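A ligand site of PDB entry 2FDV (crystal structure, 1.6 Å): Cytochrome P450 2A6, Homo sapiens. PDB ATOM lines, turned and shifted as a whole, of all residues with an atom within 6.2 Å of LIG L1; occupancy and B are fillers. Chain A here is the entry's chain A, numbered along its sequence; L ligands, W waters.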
ATOM      1  N   PHE A  85     -13.188   5.029 -11.577  1.00  0.00           N
ATOM      2  CA  PHE A  85     -12.028   5.152 -10.656  1.00  0.00           C
ATOM      3  C   PHE A  85     -11.424   3.819 -10.344  1.00  0.00           C
ATOM      4  O   PHE A  85     -10.161   3.687 -10.198  1.00  0.00           O
ATOM      5  CB  PHE A  85     -12.479   5.882  -9.351  1.00  0.00           C
ATOM      6  CG  PHE A  85     -12.984   7.274  -9.618  1.00  0.00           C
ATOM      7  CD1 PHE A  85     -14.280   7.658  -9.203  1.00  0.00           C
ATOM      8  CD2 PHE A  85     -12.222   8.200 -10.337  1.00  0.00           C
ATOM      9  CE1 PHE A  85     -14.761   8.939  -9.527  1.00  0.00           C
ATOM     10  CE2 PHE A  85     -12.734   9.487 -10.667  1.00  0.00           C
ATOM     11  CZ  PHE A  85     -14.043   9.841 -10.232  1.00  0.00           C
ATOM     12  N   PHE A  89      -7.577   2.377  -9.527  1.00  0.00           N
ATOM     13  CA  PHE A  89      -7.329   1.963  -8.156  1.00  0.00           C
ATOM     14  C   PHE A  89      -7.279   0.501  -7.895  1.00  0.00           C
ATOM     15  O   PHE A  89      -6.517   0.068  -7.024  1.00  0.00           O
ATOM     16  CB  PHE A  89      -8.334   2.674  -7.214  1.00  0.00           C
ATOM     17  CG  PHE A  89      -8.061   4.124  -7.104  1.00  0.00           C
ATOM     18  CD1 PHE A  89      -8.770   5.045  -7.835  1.00  0.00           C
ATOM     19  CD2 PHE A  89      -6.985   4.602  -6.323  1.00  0.00           C
ATOM     20  CE1 PHE A  89      -8.437   6.391  -7.816  1.00  0.00           C
ATOM     21  CE2 PHE A  89      -6.632   5.932  -6.289  1.00  0.00           C
ATOM     22  CZ  PHE A  89      -7.351   6.867  -7.037  1.00  0.00           C
ATOM     23  N   VAL A  95      -9.861   5.221  -0.471  1.00  0.00           N
ATOM     24  CA  VAL A  95     -11.255   5.499  -0.826  1.00  0.00           C
ATOM     25  C   VAL A  95     -12.002   4.323  -1.438  1.00  0.00           C
ATOM     26  O   VAL A  95     -13.088   3.898  -0.972  1.00  0.00           O
ATOM     27  CB  VAL A  95     -11.311   6.696  -1.879  1.00  0.00           C
ATOM     28  CG1 VAL A  95     -12.795   6.908  -2.341  1.00  0.00           C
ATOM     29  CG2 VAL A  95     -10.724   8.024  -1.267  1.00  0.00           C
ATOM     30  N   PHE A  96     -11.423   3.786  -2.535  1.00  0.00           N
ATOM     31  CA  PHE A  96     -12.081   2.730  -3.298  1.00  0.00           C
ATOM     32  C   PHE A  96     -11.585   1.370  -2.924  1.00  0.00           C
ATOM     33  O   PHE A  96     -11.178   0.578  -3.793  1.00  0.00           O
ATOM     34  CB  PHE A  96     -11.873   3.053  -4.803  1.00  0.00           C
ATOM     35  CG  PHE A  96     -12.444   4.357  -5.204  1.00  0.00           C
ATOM     36  CD1 PHE A  96     -11.612   5.464  -5.475  1.00  0.00           C
ATOM     37  CD2 PHE A  96     -13.852   4.540  -5.284  1.00  0.00           C
ATOM     38  CE1 PHE A  96     -12.148   6.736  -5.813  1.00  0.00           C
ATOM     39  CE2 PHE A  96     -14.369   5.809  -5.625  1.00  0.00           C
ATOM     40  CZ  PHE A  96     -13.539   6.895  -5.887  1.00  0.00           C
ATOM     41  N   PHE A 187     -13.660  14.089 -13.736  1.00  0.00           N
ATOM     42  CA  PHE A 187     -14.961  14.338 -13.071  1.00  0.00           C
ATOM     43  C   PHE A 187     -16.022  14.601 -14.164  1.00  0.00           C
ATOM     44  O   PHE A 187     -17.144  14.162 -14.040  1.00  0.00           O
ATOM     45  CB  PHE A 187     -14.894  15.546 -12.117  1.00  0.00           C
ATOM     46  CG  PHE A 187     -14.626  15.133 -10.688  1.00  0.00           C
ATOM     47  CD1 PHE A 187     -13.446  14.469 -10.368  1.00  0.00           C
ATOM     48  CD2 PHE A 187     -15.523  15.413  -9.709  1.00  0.00           C
ATOM     49  CE1 PHE A 187     -13.196  14.076  -9.005  1.00  0.00           C
ATOM     50  CE2 PHE A 187     -15.250  15.024  -8.339  1.00  0.00           C
ATOM     51  CZ  PHE A 187     -14.087  14.368  -8.067  1.00  0.00           C
ATOM     52  N   LEU A 219      -6.460   9.419 -15.734  1.00  0.00           N
ATOM     53  CA  LEU A 219      -6.134   8.764 -14.453  1.00  0.00           C
ATOM     54  C   LEU A 219      -4.687   8.275 -14.454  1.00  0.00           C
ATOM     55  O   LEU A 219      -4.001   8.365 -13.451  1.00  0.00           O
ATOM     56  CB  LEU A 219      -6.998   7.542 -14.201  1.00  0.00           C
ATOM     57  CG  LEU A 219      -8.377   8.072 -13.879  1.00  0.00           C
ATOM     58  CD1 LEU A 219      -9.340   6.854 -13.928  1.00  0.00           C
ATOM     59  CD2 LEU A 219      -8.366   8.707 -12.466  1.00  0.00           C
ATOM     60  N   MET A 271      -1.657   5.046  -4.302  1.00  0.00           N
ATOM     61  CA  MET A 271      -3.126   5.175  -4.451  1.00  0.00           C
ATOM     62  C   MET A 271      -3.720   6.042  -3.354  1.00  0.00           C
ATOM     63  O   MET A 271      -4.598   6.870  -3.625  1.00  0.00           O
ATOM     64  CB  MET A 271      -3.822   3.815  -4.482  1.00  0.00           C
ATOM     65  CG  MET A 271      -3.343   2.992  -5.710  1.00  0.00           C
ATOM     66  SD  MET A 271      -3.553   3.971  -7.315  1.00  0.00           S
ATOM     67  CE  MET A 271      -2.671   2.841  -8.451  1.00  0.00           C
ATOM     68  N   LEU A 274      -2.814   9.598  -4.216  1.00  0.00           N
ATOM     69  CA  LEU A 274      -3.589  10.000  -5.404  1.00  0.00           C
ATOM     70  C   LEU A 274      -5.032  10.364  -4.919  1.00  0.00           C
ATOM     71  O   LEU A 274      -5.634  11.374  -5.390  1.00  0.00           O
ATOM     72  CB  LEU A 274      -3.664   8.838  -6.392  1.00  0.00           C
ATOM     73  CG  LEU A 274      -4.313   9.110  -7.744  1.00  0.00           C
ATOM     74  CD1 LEU A 274      -3.653  10.294  -8.409  1.00  0.00           C
ATOM     75  CD2 LEU A 274      -4.178   7.880  -8.636  1.00  0.00           C
ATOM     76  N   ASN A 275      -5.568   9.562  -4.004  1.00  0.00           N
ATOM     77  CA  ASN A 275      -6.933   9.829  -3.511  1.00  0.00           C
ATOM     78  C   ASN A 275      -7.003  11.231  -2.851  1.00  0.00           C
ATOM     79  O   ASN A 275      -7.979  11.997  -3.024  1.00  0.00           O
ATOM     80  CB  ASN A 275      -7.360   8.839  -2.418  1.00  0.00           C
ATOM     81  CG  ASN A 275      -7.768   7.461  -2.948  1.00  0.00           C
ATOM     82  OD1 ASN A 275      -7.469   6.439  -2.295  1.00  0.00           O
ATOM     83  ND2 ASN A 275      -8.499   7.401  -4.074  1.00  0.00           N
ATOM     84  N   LEU A 276      -6.016  11.506  -2.020  1.00  0.00           N
ATOM     85  CA  LEU A 276      -6.066  12.810  -1.324  1.00  0.00           C
ATOM     86  C   LEU A 276      -5.815  13.962  -2.272  1.00  0.00           C
ATOM     87  O   LEU A 276      -6.433  15.005  -2.168  1.00  0.00           O
ATOM     88  CB  LEU A 276      -5.046  12.833  -0.151  1.00  0.00           C
ATOM     89  CG  LEU A 276      -5.221  11.756   0.937  1.00  0.00           C
ATOM     90  CD1 LEU A 276      -4.060  11.888   1.981  1.00  0.00           C
ATOM     91  CD2 LEU A 276      -6.557  11.898   1.625  1.00  0.00           C
ATOM     92  N   ILE A 278      -6.512  14.073  -5.587  1.00  0.00           N
ATOM     93  CA  ILE A 278      -7.688  14.345  -6.440  1.00  0.00           C
ATOM     94  C   ILE A 278      -8.874  14.757  -5.549  1.00  0.00           C
ATOM     95  O   ILE A 278      -9.600  15.774  -5.839  1.00  0.00           O
ATOM     96  CB  ILE A 278      -8.070  13.119  -7.231  1.00  0.00           C
ATOM     97  CG1 ILE A 278      -6.900  12.809  -8.200  1.00  0.00           C
ATOM     98  CG2 ILE A 278      -9.366  13.390  -8.057  1.00  0.00           C
ATOM     99  CD1 ILE A 278      -7.058  11.460  -8.994  1.00  0.00           C
ATOM    100  N   GLY A 279      -9.092  13.970  -4.523  1.00  0.00           N
ATOM    101  CA  GLY A 279     -10.215  14.211  -3.568  1.00  0.00           C
ATOM    102  C   GLY A 279     -10.142  15.570  -2.933  1.00  0.00           C
ATOM    103  O   GLY A 279     -11.152  16.319  -2.850  1.00  0.00           O
ATOM    104  N   GLY A 280      -8.942  15.976  -2.523  1.00  0.00           N
ATOM    105  CA  GLY A 280      -8.761  17.265  -1.911  1.00  0.00           C
ATOM    106  C   GLY A 280      -8.801  18.438  -2.837  1.00  0.00           C
ATOM    107  O   GLY A 280      -8.725  19.568  -2.391  1.00  0.00           O
ATOM    108  N   THR A 283     -13.545  18.456  -5.616  1.00  0.00           N
ATOM    109  CA  THR A 283     -14.892  18.759  -5.111  1.00  0.00           C
ATOM    110  C   THR A 283     -14.965  20.137  -4.505  1.00  0.00           C
ATOM    111  O   THR A 283     -15.998  20.823  -4.700  1.00  0.00           O
ATOM    112  CB  THR A 283     -15.342  17.731  -4.122  1.00  0.00           C
ATOM    113  OG1 THR A 283     -14.387  17.666  -3.072  1.00  0.00           O
ATOM    114  CG2 THR A 283     -15.357  16.337  -4.809  1.00  0.00           C
ATOM    115  N   ILE A 344     -21.761  15.685  -5.284  1.00  0.00           N
ATOM    116  CA  ILE A 344     -21.591  14.207  -5.427  1.00  0.00           C
ATOM    117  C   ILE A 344     -23.044  13.745  -5.159  1.00  0.00           C
ATOM    118  O   ILE A 344     -23.386  13.310  -4.065  1.00  0.00           O
ATOM    119  CB  ILE A 344     -20.623  13.657  -4.354  1.00  0.00           C
ATOM    120  CG1 ILE A 344     -19.252  14.423  -4.423  1.00  0.00           C
ATOM    121  CG2 ILE A 344     -20.428  12.123  -4.599  1.00  0.00           C
ATOM    122  CD1 ILE A 344     -18.470  14.178  -5.779  1.00  0.00           C
ATOM    123  N   LEU A 348     -20.572   8.145  -2.875  1.00  0.00           N
ATOM    124  CA  LEU A 348     -19.666   7.089  -3.417  1.00  0.00           C
ATOM    125  C   LEU A 348     -20.466   5.833  -2.913  1.00  0.00           C
ATOM    126  O   LEU A 348     -20.912   5.786  -1.719  1.00  0.00           O
ATOM    127  CB  LEU A 348     -18.238   7.141  -2.814  1.00  0.00           C
ATOM    128  CG  LEU A 348     -17.299   8.081  -3.597  1.00  0.00           C
ATOM    129  CD1 LEU A 348     -17.815   9.495  -3.627  1.00  0.00           C
ATOM    130  CD2 LEU A 348     -15.935   8.010  -2.868  1.00  0.00           C
ATOM    131  N   CYS A 417     -17.010  11.306   4.509  1.00  0.00           N
ATOM    132  CA  CYS A 417     -15.835  12.088   4.092  1.00  0.00           C
ATOM    133  C   CYS A 417     -14.945  12.514   5.249  1.00  0.00           C
ATOM    134  O   CYS A 417     -15.388  13.317   6.073  1.00  0.00           O
ATOM    135  CB  CYS A 417     -16.337  13.367   3.375  1.00  0.00           C
ATOM    136  SG  CYS A 417     -14.918  14.334   2.682  1.00  0.00           S
ATOM    137  N   PHE A 458     -21.826  10.957 -11.786  1.00  0.00           N
ATOM    138  CA  PHE A 458     -21.105  10.772 -10.524  1.00  0.00           C
ATOM    139  C   PHE A 458     -21.025  12.140  -9.788  1.00  0.00           C
ATOM    140  O   PHE A 458     -21.037  12.222  -8.517  1.00  0.00           O
ATOM    141  CB  PHE A 458     -19.672  10.269 -10.790  1.00  0.00           C
ATOM    142  CG  PHE A 458     -18.828  10.238  -9.569  1.00  0.00           C
ATOM    143  CD1 PHE A 458     -19.097   9.299  -8.573  1.00  0.00           C
ATOM    144  CD2 PHE A 458     -17.880  11.231  -9.371  1.00  0.00           C
ATOM    145  CE1 PHE A 458     -18.361   9.410  -7.341  1.00  0.00           C
ATOM    146  CE2 PHE A 458     -17.196  11.337  -8.203  1.00  0.00           C
ATOM    147  CZ  PHE A 458     -17.436  10.442  -7.196  1.00  0.00           C
HETATM  148  C1  LIG L   1     -11.935  10.651  -5.856  1.00  0.00           C
HETATM  149  C2  LIG L   1     -11.791  10.507  -7.265  1.00  0.00           C
HETATM  150  C3  LIG L   1     -10.567   9.950  -7.762  1.00  0.00           C
HETATM  151  C4  LIG L   1      -9.589   9.562  -6.803  1.00  0.00           C
HETATM  152  N1  LIG L   1      -9.747   9.694  -5.466  1.00  0.00           N
HETATM  153  C5  LIG L   1     -10.875  10.225  -4.985  1.00  0.00           C
HETATM  154  C6  LIG L   1     -13.132  11.210  -5.322  1.00  0.00           C
HETATM  155  C7  LIG L   1     -14.274  11.664  -5.895  1.00  0.00           C
HETATM  156  C8  LIG L   1     -15.136  12.123  -4.819  1.00  0.00           C
HETATM  157  C9  LIG L   1     -14.428  11.899  -3.662  1.00  0.00           C
HETATM  158  O1  LIG L   1     -13.190  11.340  -3.938  1.00  0.00           O
HETATM  159  C10 LIG L   1     -14.749  12.151  -2.187  1.00  0.00           C
HETATM  160  N2  LIG L   1     -14.247  13.409  -1.653  1.00  0.00           N
HETATM  161  C11 LIG L   1     -13.893  14.500  -2.470  1.00  0.00           C
HETATM  162  C1  LG2 L   2     -15.418  10.456   0.859  1.00  0.00           C
HETATM  163  C2  LG2 L   2     -17.872  14.435  -0.355  1.00  0.00           C
HETATM  164  C3  LG2 L   2     -13.908  17.076   0.218  1.00  0.00           C
HETATM  165  C4  LG2 L   2     -11.379  13.081   1.013  1.00  0.00           C
HETATM  166  C5  LG2 L   2     -16.456  11.305   0.460  1.00  0.00           C
HETATM  167  C6  LG2 L   2     -17.783  10.918   0.202  1.00  0.00           C
HETATM  168  C7  LG2 L   2     -18.465  12.053  -0.132  1.00  0.00           C
HETATM  169  C8  LG2 L   2     -17.578  13.109  -0.061  1.00  0.00           C
HETATM  170  C9  LG2 L   2     -19.977  12.162  -0.531  1.00  0.00           C
HETATM  171  C10 LG2 L   2     -18.273   9.498   0.308  1.00  0.00           C
HETATM  172  C11 LG2 L   2     -18.669   9.243   1.786  1.00  0.00           C
HETATM  173  C12 LG2 L   2     -19.298   7.896   2.042  1.00  0.00           C
HETATM  174  O1  LG2 L   2     -20.309   7.879   2.809  1.00  0.00           O
HETATM  175  O2  LG2 L   2     -18.966   6.839   1.437  1.00  0.00           O
HETATM  176  C13 LG2 L   2     -16.982  15.547  -0.460  1.00  0.00           C
HETATM  177  C14 LG2 L   2     -17.310  16.875  -0.709  1.00  0.00           C
HETATM  178  C15 LG2 L   2     -16.209  17.614  -0.500  1.00  0.00           C
HETATM  179  C16 LG2 L   2     -15.186  16.688  -0.118  1.00  0.00           C
HETATM  180  C17 LG2 L   2     -18.714  17.371  -1.098  1.00  0.00           C
HETATM  181  C18 LG2 L   2     -16.016  19.026  -0.597  1.00  0.00           C
HETATM  182  C19 LG2 L   2     -16.938  20.145  -0.940  1.00  0.00           C
HETATM  183  C20 LG2 L   2     -12.844  16.259   0.556  1.00  0.00           C
HETATM  184  C21 LG2 L   2     -11.512  16.687   0.798  1.00  0.00           C
HETATM  185  C22 LG2 L   2     -10.769  15.537   0.949  1.00  0.00           C
HETATM  186  C23 LG2 L   2     -11.662  14.458   0.805  1.00  0.00           C
HETATM  187  C24 LG2 L   2     -10.973  18.151   0.894  1.00  0.00           C
HETATM  188  C25 LG2 L   2      -9.409  15.337   1.196  1.00  0.00           C
HETATM  189  C26 LG2 L   2      -8.523  15.999   2.014  1.00  0.00           C
HETATM  190  C27 LG2 L   2     -12.253  12.003   1.050  1.00  0.00           C
HETATM  191  C28 LG2 L   2     -11.887  10.658   1.301  1.00  0.00           C
HETATM  192  C29 LG2 L   2     -13.017   9.899   1.257  1.00  0.00           C
HETATM  193  C30 LG2 L   2     -14.064  10.819   0.989  1.00  0.00           C
HETATM  194  C31 LG2 L   2     -10.451  10.117   1.549  1.00  0.00           C
HETATM  195  C32 LG2 L   2     -13.187   8.424   1.435  1.00  0.00           C
HETATM  196  C33 LG2 L   2     -13.550   8.011   2.900  1.00  0.00           C
HETATM  197  C34 LG2 L   2     -13.656   6.455   3.049  1.00  0.00           C
HETATM  198  O3  LG2 L   2     -13.492   5.940   4.125  1.00  0.00           O
HETATM  199  O4  LG2 L   2     -13.852   5.734   2.058  1.00  0.00           O
HETATM  200  N1  LG2 L   2     -16.332  12.675   0.297  1.00  0.00           N
HETATM  201  N2  LG2 L   2     -15.667  15.457  -0.093  1.00  0.00           N
HETATM  202  N3  LG2 L   2     -12.938  14.909   0.555  1.00  0.00           N
HETATM  203  N4  LG2 L   2     -13.574  12.067   0.873  1.00  0.00           N
HETATM  204 FE1  LG2 L   2     -14.620  13.786   0.464  1.00  0.00          FE
HETATM  205  O   HOH W   1     -12.389  16.008  -5.032  1.00  0.00           O
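The side-chain amide nitrogen (ND2) of Asn 275 sits at hydrogen-bond distance from a nitrogen (N1) of LIG L1 (3.0 Å).
The side-chain sulfur (SG) of Cys 417 binds an iron atom (FE1) of LG2 L2.
N2 of LIG L1 binds FE1 of LG2 L2, 2.2 Å away.
OD1 of Asn 275 lies close to O of Met 271, at 3.2 Å.
The side-chain amide oxygen (OD1) of Asn 275 sits at hydrogen-bond distance from the backbone NH (N) of Val 95 (3.2 Å).
CD2 of Phe 85 touches C3 of LIG L1, at 3.5 Å.
Phe 89 touches LIG L1.
Phe 96 touches LIG L1 (CE1 to C5, 3.8 Å).
Phe 187 touches LIG L1 (CZ to C7, 3.5 Å).
Ile 278 touches LIG L1 (CG2 to C3, 3.7 Å).
Gly 279 touches LIG L1.
OG1 of Thr 283 touches C11 of LIG L1 (3.3 Å).
Leu 348 touches LIG L1.
Phe 458 touches LIG L1 (CZ to C7, 3.6 Å).
Hydrophobic or aromatic side chains within 4 Å of LIG L1: Phe 85, Phe 89, Phe 96, Phe 187, Ile 278, Leu 348 and Phe 458.
Of the 18 residues printed, 10 come within 4 Å of LIG L1.
Water W1 lies within hydrogen-bond range of O of Gly 279 (2.5 Å), N of Thr 283 (2.8 Å) and O of Ile 278 (2.9 Å).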
